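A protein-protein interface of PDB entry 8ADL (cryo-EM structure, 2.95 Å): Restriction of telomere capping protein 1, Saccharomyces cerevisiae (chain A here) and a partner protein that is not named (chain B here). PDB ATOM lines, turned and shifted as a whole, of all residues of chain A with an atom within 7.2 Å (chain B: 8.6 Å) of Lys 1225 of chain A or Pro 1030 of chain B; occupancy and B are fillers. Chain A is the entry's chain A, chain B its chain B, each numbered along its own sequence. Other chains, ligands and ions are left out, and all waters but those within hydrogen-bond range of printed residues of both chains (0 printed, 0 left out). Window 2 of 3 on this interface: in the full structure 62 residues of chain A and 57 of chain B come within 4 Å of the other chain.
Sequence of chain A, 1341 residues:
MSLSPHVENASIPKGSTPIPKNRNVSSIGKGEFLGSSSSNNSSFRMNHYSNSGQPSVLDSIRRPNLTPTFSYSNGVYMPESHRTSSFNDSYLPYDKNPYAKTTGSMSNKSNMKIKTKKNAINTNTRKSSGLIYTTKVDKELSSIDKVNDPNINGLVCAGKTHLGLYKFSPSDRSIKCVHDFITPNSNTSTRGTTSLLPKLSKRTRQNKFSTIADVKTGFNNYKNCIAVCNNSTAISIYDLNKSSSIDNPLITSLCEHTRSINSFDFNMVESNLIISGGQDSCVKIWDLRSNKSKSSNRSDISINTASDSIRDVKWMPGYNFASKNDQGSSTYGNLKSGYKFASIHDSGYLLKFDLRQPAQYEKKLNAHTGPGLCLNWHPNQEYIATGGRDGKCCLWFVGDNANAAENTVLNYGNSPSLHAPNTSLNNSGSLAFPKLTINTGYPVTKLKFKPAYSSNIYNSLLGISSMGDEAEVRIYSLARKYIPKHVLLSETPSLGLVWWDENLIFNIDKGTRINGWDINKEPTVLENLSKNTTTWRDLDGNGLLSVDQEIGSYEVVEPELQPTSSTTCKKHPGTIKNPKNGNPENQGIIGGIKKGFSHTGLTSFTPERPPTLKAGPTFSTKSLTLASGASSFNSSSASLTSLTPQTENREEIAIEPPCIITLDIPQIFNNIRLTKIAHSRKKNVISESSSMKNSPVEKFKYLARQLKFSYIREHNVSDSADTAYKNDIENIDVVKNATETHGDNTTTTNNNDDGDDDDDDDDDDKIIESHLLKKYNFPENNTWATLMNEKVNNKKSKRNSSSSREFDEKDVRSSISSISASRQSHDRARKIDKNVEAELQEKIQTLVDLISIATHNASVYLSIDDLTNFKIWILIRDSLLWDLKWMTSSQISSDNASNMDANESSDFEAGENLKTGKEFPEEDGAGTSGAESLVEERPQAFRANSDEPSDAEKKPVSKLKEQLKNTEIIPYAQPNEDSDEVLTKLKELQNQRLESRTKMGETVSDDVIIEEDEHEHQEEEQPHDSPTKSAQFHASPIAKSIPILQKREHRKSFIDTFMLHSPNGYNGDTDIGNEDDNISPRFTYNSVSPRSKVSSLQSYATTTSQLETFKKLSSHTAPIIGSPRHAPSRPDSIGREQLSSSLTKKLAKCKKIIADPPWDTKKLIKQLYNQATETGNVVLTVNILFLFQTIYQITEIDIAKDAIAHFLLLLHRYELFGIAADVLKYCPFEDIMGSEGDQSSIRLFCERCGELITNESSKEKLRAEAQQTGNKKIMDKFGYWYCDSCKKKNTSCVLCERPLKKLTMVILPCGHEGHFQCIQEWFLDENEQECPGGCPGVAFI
Lys 1225 of chain A touches just these residues of chain B: Val 1026, Cys 1027, Pro 1028, Thr 1029, Pro 1030 and Cys 1032. Pro 1030 of chain B touches two residues of chain A. Printed residues of chain B within 4 Å of Asp 1222 of chain A: Trp 1020 and His 1024. Printed residues of chain A within 4 Å of His 1024 of chain B: Asp 1222 (2.8 Å). Of the printed residues of chain B, Leu 1224 of chain A touches Pro 1030. Of the printed residues of chain A, Val 1026 of chain B touches Lys 1225. Of the printed residues of chain A, Trp 1020 of chain B touches Ala 1221 and Asp 1222. Ser 710 of chain A touches none of the printed residues of chain B. Gly 1031 of chain B touches none of the printed residues of chain A. The nearest residue of chain A that does not touch Pro 1030 of chain B is Asp 1238 of chain A (5.3 Å).
Of the 15 printed residues of chain A, 4 touch a printed residue of chain B. Of the 15 printed residues of chain B, 8 touch a printed residue of chain A. Printed residues of chain B that touch a printed residue of chain A: Trp 1020, His 1024, Val 1026, Cys 1027, Pro 1028, Thr 1029, Pro 1030 and Cys 1032. Among the printed residues, 10 pairs touch across the chains.
CB of Ala 1221 of chain A touches CZ3 of Trp 1020 of chain B, 3.7 Å away. Trp 1020 of chain B touches Asp 1222 of chain A (CH2 to OD1, 3.2 Å). O of Leu 1224 of chain A touches CB of Pro 1030 of chain B (3.9 Å). Lys 1225 of chain A touches Val 1026 of chain B (CE to CG1, 3.7 Å). Lys 1225 of chain A touches Pro 1028 of chain B. Lys 1225 of chain A touches Pro 1030 of chain B (O to CB, 3.7 Å).
The side-chain carboxylate of Asp 1222 of chain A is in hydrogen-bond range of a ring nitrogen (NE2) of His 1024 of chain B (2.8 Å). The side-chain amino group of Lys 1225 of chain A is in hydrogen-bond range of the backbone carbonyl oxygen of Cys 1027 of chain B (2.7 Å). The backbone carbonyl oxygen (O) of Thr 1029 of chain B sits at hydrogen-bond distance from the side-chain amino group (NZ) of Lys 1225 of chain A (3.1 Å). NZ of Lys 1225 of chain A lies within hydrogen-bond range of O of Cys 1032 of chain B.
A ring nitrogen (ND1) of His 1010 of chain B sits close to the side-chain hydroxyl (OG1) of Thr 1029 of chain B, 3.1 Å away. ND1 of His 1024 of chain B is in hydrogen-bond range of O of Trp 1020 of chain B (2.9 Å). NE1 of Trp 1020 of chain B sits at hydrogen-bond distance from O of Val 1026 of chain B. The side-chain sulfur (SG) of Cys 1027 of chain B lies close to the side-chain hydroxyl (OG1) of Thr 1029 of chain B (3.3 Å). N of Cys 1027 of chain B sits at hydrogen-bond distance from O of Cys 1034 of chain B (3.3 Å).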
ATOM      1  N   SER A 710      -0.267  16.101  -9.728  1.00  0.00           N
ATOM      2  CA  SER A 710      -1.536  15.475 -10.063  1.00  0.00           C
ATOM      3  C   SER A 710      -2.009  15.923 -11.438  1.00  0.00           C
ATOM      4  O   SER A 710      -1.933  17.105 -11.781  1.00  0.00           O
ATOM      5  CB  SER A 710      -2.598  15.813  -9.015  1.00  0.00           C
ATOM      6  OG  SER A 710      -2.108  15.592  -7.704  1.00  0.00           O
ATOM      7  N   LEU A1208       6.447   8.701  -0.681  1.00  0.00           N
ATOM      8  CA  LEU A1208       5.528   9.060   0.394  1.00  0.00           C
ATOM      9  C   LEU A1208       6.129   8.768   1.764  1.00  0.00           C
ATOM     10  O   LEU A1208       5.921   9.535   2.712  1.00  0.00           O
ATOM     11  CB  LEU A1208       4.202   8.331   0.210  1.00  0.00           C
ATOM     12  CG  LEU A1208       3.314   8.985  -0.846  1.00  0.00           C
ATOM     13  CD1 LEU A1208       2.325   7.991  -1.407  1.00  0.00           C
ATOM     14  CD2 LEU A1208       2.594  10.177  -0.248  1.00  0.00           C
ATOM     15  N   ILE A1219       1.615  17.691   2.390  1.00  0.00           N
ATOM     16  CA  ILE A1219       2.110  17.437   1.040  1.00  0.00           C
ATOM     17  C   ILE A1219       1.910  15.973   0.666  1.00  0.00           C
ATOM     18  O   ILE A1219       1.502  15.655  -0.459  1.00  0.00           O
ATOM     19  CB  ILE A1219       3.589  17.853   0.935  1.00  0.00           C
ATOM     20  CG1 ILE A1219       3.755  19.321   1.333  1.00  0.00           C
ATOM     21  CG2 ILE A1219       4.105  17.622  -0.468  1.00  0.00           C
ATOM     22  CD1 ILE A1219       5.183  19.814   1.279  1.00  0.00           C
ATOM     23  N   ALA A1220       2.179  15.061   1.605  1.00  0.00           N
ATOM     24  CA  ALA A1220       1.942  13.643   1.360  1.00  0.00           C
ATOM     25  C   ALA A1220       0.459  13.345   1.180  1.00  0.00           C
ATOM     26  O   ALA A1220       0.096  12.471   0.385  1.00  0.00           O
ATOM     27  CB  ALA A1220       2.516  12.806   2.501  1.00  0.00           C
ATOM     28  N   ALA A1221      -0.407  14.068   1.896  1.00  0.00           N
ATOM     29  CA  ALA A1221      -1.846  13.911   1.711  1.00  0.00           C
ATOM     30  C   ALA A1221      -2.281  14.393   0.333  1.00  0.00           C
ATOM     31  O   ALA A1221      -3.115  13.752  -0.317  1.00  0.00           O
ATOM     32  CB  ALA A1221      -2.601  14.657   2.808  1.00  0.00           C
ATOM     33  N   ASP A1222      -1.724  15.522  -0.123  1.00  0.00           N
ATOM     34  CA  ASP A1222      -1.987  16.006  -1.478  1.00  0.00           C
ATOM     35  C   ASP A1222      -1.523  15.004  -2.526  1.00  0.00           C
ATOM     36  O   ASP A1222      -2.197  14.798  -3.543  1.00  0.00           O
ATOM     37  CB  ASP A1222      -1.292  17.350  -1.701  1.00  0.00           C
ATOM     38  CG  ASP A1222      -2.044  18.506  -1.085  1.00  0.00           C
ATOM     39  OD1 ASP A1222      -3.290  18.475  -1.092  1.00  0.00           O
ATOM     40  OD2 ASP A1222      -1.388  19.450  -0.595  1.00  0.00           O
ATOM     41  N   VAL A1223      -0.359  14.393  -2.303  1.00  0.00           N
ATOM     42  CA  VAL A1223       0.179  13.410  -3.239  1.00  0.00           C
ATOM     43  C   VAL A1223      -0.697  12.159  -3.282  1.00  0.00           C
ATOM     44  O   VAL A1223      -1.028  11.654  -4.362  1.00  0.00           O
ATOM     45  CB  VAL A1223       1.637  13.089  -2.861  1.00  0.00           C
ATOM     46  CG1 VAL A1223       2.118  11.842  -3.551  1.00  0.00           C
ATOM     47  CG2 VAL A1223       2.540  14.256  -3.229  1.00  0.00           C
ATOM     48  N   LEU A1224      -1.112  11.656  -2.117  1.00  0.00           N
ATOM     49  CA  LEU A1224      -1.893  10.426  -2.056  1.00  0.00           C
ATOM     50  C   LEU A1224      -3.357  10.614  -2.443  1.00  0.00           C
ATOM     51  O   LEU A1224      -4.003   9.637  -2.843  1.00  0.00           O
ATOM     52  CB  LEU A1224      -1.802   9.830  -0.647  1.00  0.00           C
ATOM     53  CG  LEU A1224      -2.255   8.385  -0.421  1.00  0.00           C
ATOM     54  CD1 LEU A1224      -1.339   7.405  -1.128  1.00  0.00           C
ATOM     55  CD2 LEU A1224      -2.333   8.073   1.065  1.00  0.00           C
ATOM     56  N   LYS A1225      -3.896  11.835  -2.346  1.00  0.00           N
ATOM     57  CA  LYS A1225      -5.310  12.051  -2.644  1.00  0.00           C
ATOM     58  C   LYS A1225      -5.621  11.846  -4.121  1.00  0.00           C
ATOM     59  O   LYS A1225      -6.666  11.283  -4.468  1.00  0.00           O
ATOM     60  CB  LYS A1225      -5.725  13.453  -2.205  1.00  0.00           C
ATOM     61  CG  LYS A1225      -7.222  13.622  -2.036  1.00  0.00           C
ATOM     62  CD  LYS A1225      -7.597  15.081  -1.862  1.00  0.00           C
ATOM     63  CE  LYS A1225      -9.057  15.309  -2.201  1.00  0.00           C
ATOM     64  NZ  LYS A1225      -9.923  14.223  -1.664  1.00  0.00           N
ATOM     65  N   TYR A1226      -4.730  12.289  -5.006  1.00  0.00           N
ATOM     66  CA  TYR A1226      -4.944  12.204  -6.446  1.00  0.00           C
ATOM     67  C   TYR A1226      -3.974  11.234  -7.112  1.00  0.00           C
ATOM     68  O   TYR A1226      -3.574  11.435  -8.261  1.00  0.00           O
ATOM     69  CB  TYR A1226      -4.841  13.589  -7.080  1.00  0.00           C
ATOM     70  CG  TYR A1226      -5.826  14.587  -6.518  1.00  0.00           C
ATOM     71  CD1 TYR A1226      -7.195  14.383  -6.635  1.00  0.00           C
ATOM     72  CD2 TYR A1226      -5.386  15.736  -5.870  1.00  0.00           C
ATOM     73  CE1 TYR A1226      -8.099  15.293  -6.123  1.00  0.00           C
ATOM     74  CE2 TYR A1226      -6.283  16.652  -5.355  1.00  0.00           C
ATOM     75  CZ  TYR A1226      -7.638  16.425  -5.485  1.00  0.00           C
ATOM     76  OH  TYR A1226      -8.534  17.334  -4.973  1.00  0.00           O
ATOM     77  N   CYS A1227      -3.592  10.185  -6.403  1.00  0.00           N
ATOM     78  CA  CYS A1227      -2.691   9.184  -6.957  1.00  0.00           C
ATOM     79  C   CYS A1227      -3.465   8.245  -7.875  1.00  0.00           C
ATOM     80  O   CYS A1227      -4.499   7.706  -7.466  1.00  0.00           O
ATOM     81  CB  CYS A1227      -2.023   8.391  -5.840  1.00  0.00           C
ATOM     82  SG  CYS A1227      -0.829   7.163  -6.401  1.00  0.00           S
ATOM     83  N   PRO A1228      -3.014   8.042  -9.118  1.00  0.00           N
ATOM     84  CA  PRO A1228      -3.713   7.100 -10.012  1.00  0.00           C
ATOM     85  C   PRO A1228      -3.640   5.651  -9.560  1.00  0.00           C
ATOM     86  O   PRO A1228      -4.469   4.845  -9.998  1.00  0.00           O
ATOM     87  CB  PRO A1228      -3.003   7.298 -11.357  1.00  0.00           C
ATOM     88  CG  PRO A1228      -1.677   7.886 -11.008  1.00  0.00           C
ATOM     89  CD  PRO A1228      -1.909   8.735  -9.799  1.00  0.00           C
ATOM     90  N   GLU A1230      -4.338   3.061  -6.720  1.00  0.00           N
ATOM     91  CA  GLU A1230      -5.280   3.119  -5.610  1.00  0.00           C
ATOM     92  C   GLU A1230      -4.825   2.353  -4.375  1.00  0.00           C
ATOM     93  O   GLU A1230      -5.477   2.458  -3.331  1.00  0.00           O
ATOM     94  CB  GLU A1230      -6.645   2.586  -6.058  1.00  0.00           C
ATOM     95  CG  GLU A1230      -6.642   1.111  -6.426  1.00  0.00           C
ATOM     96  CD  GLU A1230      -6.488   0.884  -7.917  1.00  0.00           C
ATOM     97  OE1 GLU A1230      -6.440   1.880  -8.670  1.00  0.00           O
ATOM     98  OE2 GLU A1230      -6.412  -0.289  -8.337  1.00  0.00           O
ATOM     99  N   GLY A1237      -8.509  -0.085   2.494  1.00  0.00           N
ATOM    100  CA  GLY A1237      -9.450   0.891   1.981  1.00  0.00           C
ATOM    101  C   GLY A1237      -9.568   2.111   2.871  1.00  0.00           C
ATOM    102  O   GLY A1237      -8.631   2.907   2.974  1.00  0.00           O
ATOM    103  N   ASP A1238     -10.720   2.265   3.521  1.00  0.00           N
ATOM    104  CA  ASP A1238     -10.974   3.404   4.401  1.00  0.00           C
ATOM    105  C   ASP A1238     -10.427   3.062   5.779  1.00  0.00           C
ATOM    106  O   ASP A1238     -11.093   2.428   6.599  1.00  0.00           O
ATOM    107  CB  ASP A1238     -12.461   3.733   4.445  1.00  0.00           C
ATOM    108  CG  ASP A1238     -12.991   4.222   3.111  1.00  0.00           C
ATOM    109  OD1 ASP A1238     -12.185   4.379   2.170  1.00  0.00           O
ATOM    110  OD2 ASP A1238     -14.214   4.449   3.004  1.00  0.00           O
ATOM    111  N   ALA B 954      -6.028  10.885   8.749  1.00  0.00           N
ATOM    112  CA  ALA B 954      -6.052  10.975   7.296  1.00  0.00           C
ATOM    113  C   ALA B 954      -4.856  11.721   6.721  1.00  0.00           C
ATOM    114  O   ALA B 954      -4.655  11.686   5.502  1.00  0.00           O
ATOM    115  CB  ALA B 954      -7.342  11.654   6.835  1.00  0.00           C
ATOM    116  N   LEU B 957      -1.334   9.307   8.900  1.00  0.00           N
ATOM    117  CA  LEU B 957      -1.549   7.855   8.962  1.00  0.00           C
ATOM    118  C   LEU B 957      -1.072   7.246  10.280  1.00  0.00           C
ATOM    119  O   LEU B 957      -0.696   6.073  10.336  1.00  0.00           O
ATOM    120  CB  LEU B 957      -0.907   7.132   7.774  1.00  0.00           C
ATOM    121  CG  LEU B 957      -1.361   7.596   6.391  1.00  0.00           C
ATOM    122  CD1 LEU B 957      -0.722   6.741   5.318  1.00  0.00           C
ATOM    123  CD2 LEU B 957      -2.875   7.563   6.277  1.00  0.00           C
ATOM    124  N   HIS B1010     -14.458  10.927   8.577  1.00  0.00           N
ATOM    125  CA  HIS B1010     -13.031  10.750   8.347  1.00  0.00           C
ATOM    126  C   HIS B1010     -12.251  11.491   9.421  1.00  0.00           C
ATOM    127  O   HIS B1010     -12.476  12.683   9.648  1.00  0.00           O
ATOM    128  CB  HIS B1010     -12.636  11.235   6.952  1.00  0.00           C
ATOM    129  CG  HIS B1010     -13.051  10.303   5.857  1.00  0.00           C
ATOM    130  ND1 HIS B1010     -13.576  10.744   4.662  1.00  0.00           N
ATOM    131  CD2 HIS B1010     -13.028   8.952   5.782  1.00  0.00           C
ATOM    132  CE1 HIS B1010     -13.858   9.704   3.897  1.00  0.00           C
ATOM    133  NE2 HIS B1010     -13.532   8.605   4.554  1.00  0.00           N
ATOM    134  N   TRP B1020      -4.370  21.442   7.267  1.00  0.00           N
ATOM    135  CA  TRP B1020      -4.832  20.990   5.958  1.00  0.00           C
ATOM    136  C   TRP B1020      -5.862  21.939   5.360  1.00  0.00           C
ATOM    137  O   TRP B1020      -5.801  22.253   4.165  1.00  0.00           O
ATOM    138  CB  TRP B1020      -5.411  19.580   6.074  1.00  0.00           C
ATOM    139  CG  TRP B1020      -6.199  19.149   4.876  1.00  0.00           C
ATOM    140  CD1 TRP B1020      -7.555  19.192   4.728  1.00  0.00           C
ATOM    141  CD2 TRP B1020      -5.681  18.614   3.655  1.00  0.00           C
ATOM    142  NE1 TRP B1020      -7.912  18.717   3.492  1.00  0.00           N
ATOM    143  CE2 TRP B1020      -6.779  18.356   2.813  1.00  0.00           C
ATOM    144  CE3 TRP B1020      -4.394  18.329   3.190  1.00  0.00           C
ATOM    145  CZ2 TRP B1020      -6.631  17.827   1.536  1.00  0.00           C
ATOM    146  CZ3 TRP B1020      -4.250  17.802   1.924  1.00  0.00           C
ATOM    147  CH2 TRP B1020      -5.362  17.554   1.112  1.00  0.00           C
ATOM    148  N   HIS B1024      -6.516  23.961   1.640  1.00  0.00           N
ATOM    149  CA  HIS B1024      -7.413  23.185   0.794  1.00  0.00           C
ATOM    150  C   HIS B1024      -8.847  23.296   1.303  1.00  0.00           C
ATOM    151  O   HIS B1024      -9.128  23.944   2.313  1.00  0.00           O
ATOM    152  CB  HIS B1024      -6.971  21.720   0.734  1.00  0.00           C
ATOM    153  CG  HIS B1024      -5.499  21.541   0.535  1.00  0.00           C
ATOM    154  ND1 HIS B1024      -4.604  21.523   1.583  1.00  0.00           N
ATOM    155  CD2 HIS B1024      -4.766  21.373  -0.590  1.00  0.00           C
ATOM    156  CE1 HIS B1024      -3.383  21.352   1.112  1.00  0.00           C
ATOM    157  NE2 HIS B1024      -3.453  21.259  -0.203  1.00  0.00           N
ATOM    158  N   ASN B1025      -9.764  22.650   0.576  1.00  0.00           N
ATOM    159  CA  ASN B1025     -11.177  22.678   0.933  1.00  0.00           C
ATOM    160  C   ASN B1025     -11.867  21.329   0.761  1.00  0.00           C
ATOM    161  O   ASN B1025     -13.100  21.274   0.832  1.00  0.00           O
ATOM    162  CB  ASN B1025     -11.913  23.736   0.099  1.00  0.00           C
ATOM    163  CG  ASN B1025     -11.805  25.124   0.694  1.00  0.00           C
ATOM    164  OD1 ASN B1025     -11.723  25.287   1.911  1.00  0.00           O
ATOM    165  ND2 ASN B1025     -11.807  26.137  -0.165  1.00  0.00           N
ATOM    166  N   VAL B1026     -11.124  20.247   0.533  1.00  0.00           N
ATOM    167  CA  VAL B1026     -11.695  18.923   0.319  1.00  0.00           C
ATOM    168  C   VAL B1026     -11.102  17.995   1.375  1.00  0.00           C
ATOM    169  O   VAL B1026     -10.024  18.261   1.914  1.00  0.00           O
ATOM    170  CB  VAL B1026     -11.404  18.417  -1.122  1.00  0.00           C
ATOM    171  CG1 VAL B1026     -12.211  17.167  -1.482  1.00  0.00           C
ATOM    172  CG2 VAL B1026     -11.648  19.512  -2.154  1.00  0.00           C
ATOM    173  N   CYS B1027     -11.832  16.924   1.696  1.00  0.00           N
ATOM    174  CA  CYS B1027     -11.359  15.930   2.651  1.00  0.00           C
ATOM    175  C   CYS B1027     -10.091  15.258   2.130  1.00  0.00           C
ATOM    176  O   CYS B1027     -10.031  14.890   0.948  1.00  0.00           O
ATOM    177  CB  CYS B1027     -12.448  14.888   2.902  1.00  0.00           C
ATOM    178  SG  CYS B1027     -12.055  13.643   4.146  1.00  0.00           S
ATOM    179  N   PRO B1028      -9.060  15.089   2.965  1.00  0.00           N
ATOM    180  CA  PRO B1028      -7.783  14.544   2.468  1.00  0.00           C
ATOM    181  C   PRO B1028      -7.818  13.077   2.077  1.00  0.00           C
ATOM    182  O   PRO B1028      -6.878  12.622   1.413  1.00  0.00           O
ATOM    183  CB  PRO B1028      -6.827  14.774   3.643  1.00  0.00           C
ATOM    184  CG  PRO B1028      -7.715  14.862   4.836  1.00  0.00           C
ATOM    185  CD  PRO B1028      -8.957  15.542   4.361  1.00  0.00           C
ATOM    186  N   THR B1029      -8.835  12.319   2.474  1.00  0.00           N
ATOM    187  CA  THR B1029      -8.912  10.923   2.070  1.00  0.00           C
ATOM    188  C   THR B1029      -9.192  10.813   0.571  1.00  0.00           C
ATOM    189  O   THR B1029      -9.990  11.583   0.030  1.00  0.00           O
ATOM    190  CB  THR B1029      -9.998  10.191   2.853  1.00  0.00           C
ATOM    191  OG1 THR B1029     -11.253  10.846   2.648  1.00  0.00           O
ATOM    192  CG2 THR B1029      -9.673  10.183   4.334  1.00  0.00           C
ATOM    193  N   PRO B1030      -8.536   9.883  -0.125  1.00  0.00           N
ATOM    194  CA  PRO B1030      -8.793   9.707  -1.562  1.00  0.00           C
ATOM    195  C   PRO B1030     -10.186   9.145  -1.811  1.00  0.00           C
ATOM    196  O   PRO B1030     -10.597   8.166  -1.184  1.00  0.00           O
ATOM    197  CB  PRO B1030      -7.703   8.723  -2.002  1.00  0.00           C
ATOM    198  CG  PRO B1030      -7.288   8.029  -0.748  1.00  0.00           C
ATOM    199  CD  PRO B1030      -7.423   9.040   0.343  1.00  0.00           C
ATOM    200  N   GLY B1031     -10.910   9.770  -2.735  1.00  0.00           N
ATOM    201  CA  GLY B1031     -12.238   9.314  -3.083  1.00  0.00           C
ATOM    202  C   GLY B1031     -13.374   9.972  -2.336  1.00  0.00           C
ATOM    203  O   GLY B1031     -14.526   9.558  -2.512  1.00  0.00           O
ATOM    204  N   CYS B1032     -13.097  10.977  -1.510  1.00  0.00           N
ATOM    205  CA  CYS B1032     -14.120  11.668  -0.737  1.00  0.00           C
ATOM    206  C   CYS B1032     -14.192  13.120  -1.180  1.00  0.00           C
ATOM    207  O   CYS B1032     -13.167  13.807  -1.239  1.00  0.00           O
ATOM    208  CB  CYS B1032     -13.826  11.586   0.762  1.00  0.00           C
ATOM    209  SG  CYS B1032     -14.954  12.530   1.817  1.00  0.00           S
ATOM    210  N   THR B1033     -15.401  13.580  -1.490  1.00  0.00           N
ATOM    211  CA  THR B1033     -15.658  14.968  -1.863  1.00  0.00           C
ATOM    212  C   THR B1033     -16.588  15.548  -0.803  1.00  0.00           C
ATOM    213  O   THR B1033     -17.812  15.513  -0.946  1.00  0.00           O
ATOM    214  CB  THR B1033     -16.265  15.067  -3.259  1.00  0.00           C
ATOM    215  OG1 THR B1033     -15.477  14.299  -4.177  1.00  0.00           O
ATOM    216  CG2 THR B1033     -16.295  16.515  -3.723  1.00  0.00           C
ATOM    217  N   CYS B1034     -16.001  16.077   0.268  1.00  0.00           N
ATOM    218  CA  CYS B1034     -16.763  16.634   1.380  1.00  0.00           C
ATOM    219  C   CYS B1034     -16.005  17.844   1.906  1.00  0.00           C
ATOM    220  O   CYS B1034     -14.911  17.700   2.459  1.00  0.00           O
ATOM    221  CB  CYS B1034     -16.979  15.595   2.481  1.00  0.00           C
ATOM    222  SG  CYS B1034     -17.708  16.246   4.000  1.00  0.00           S
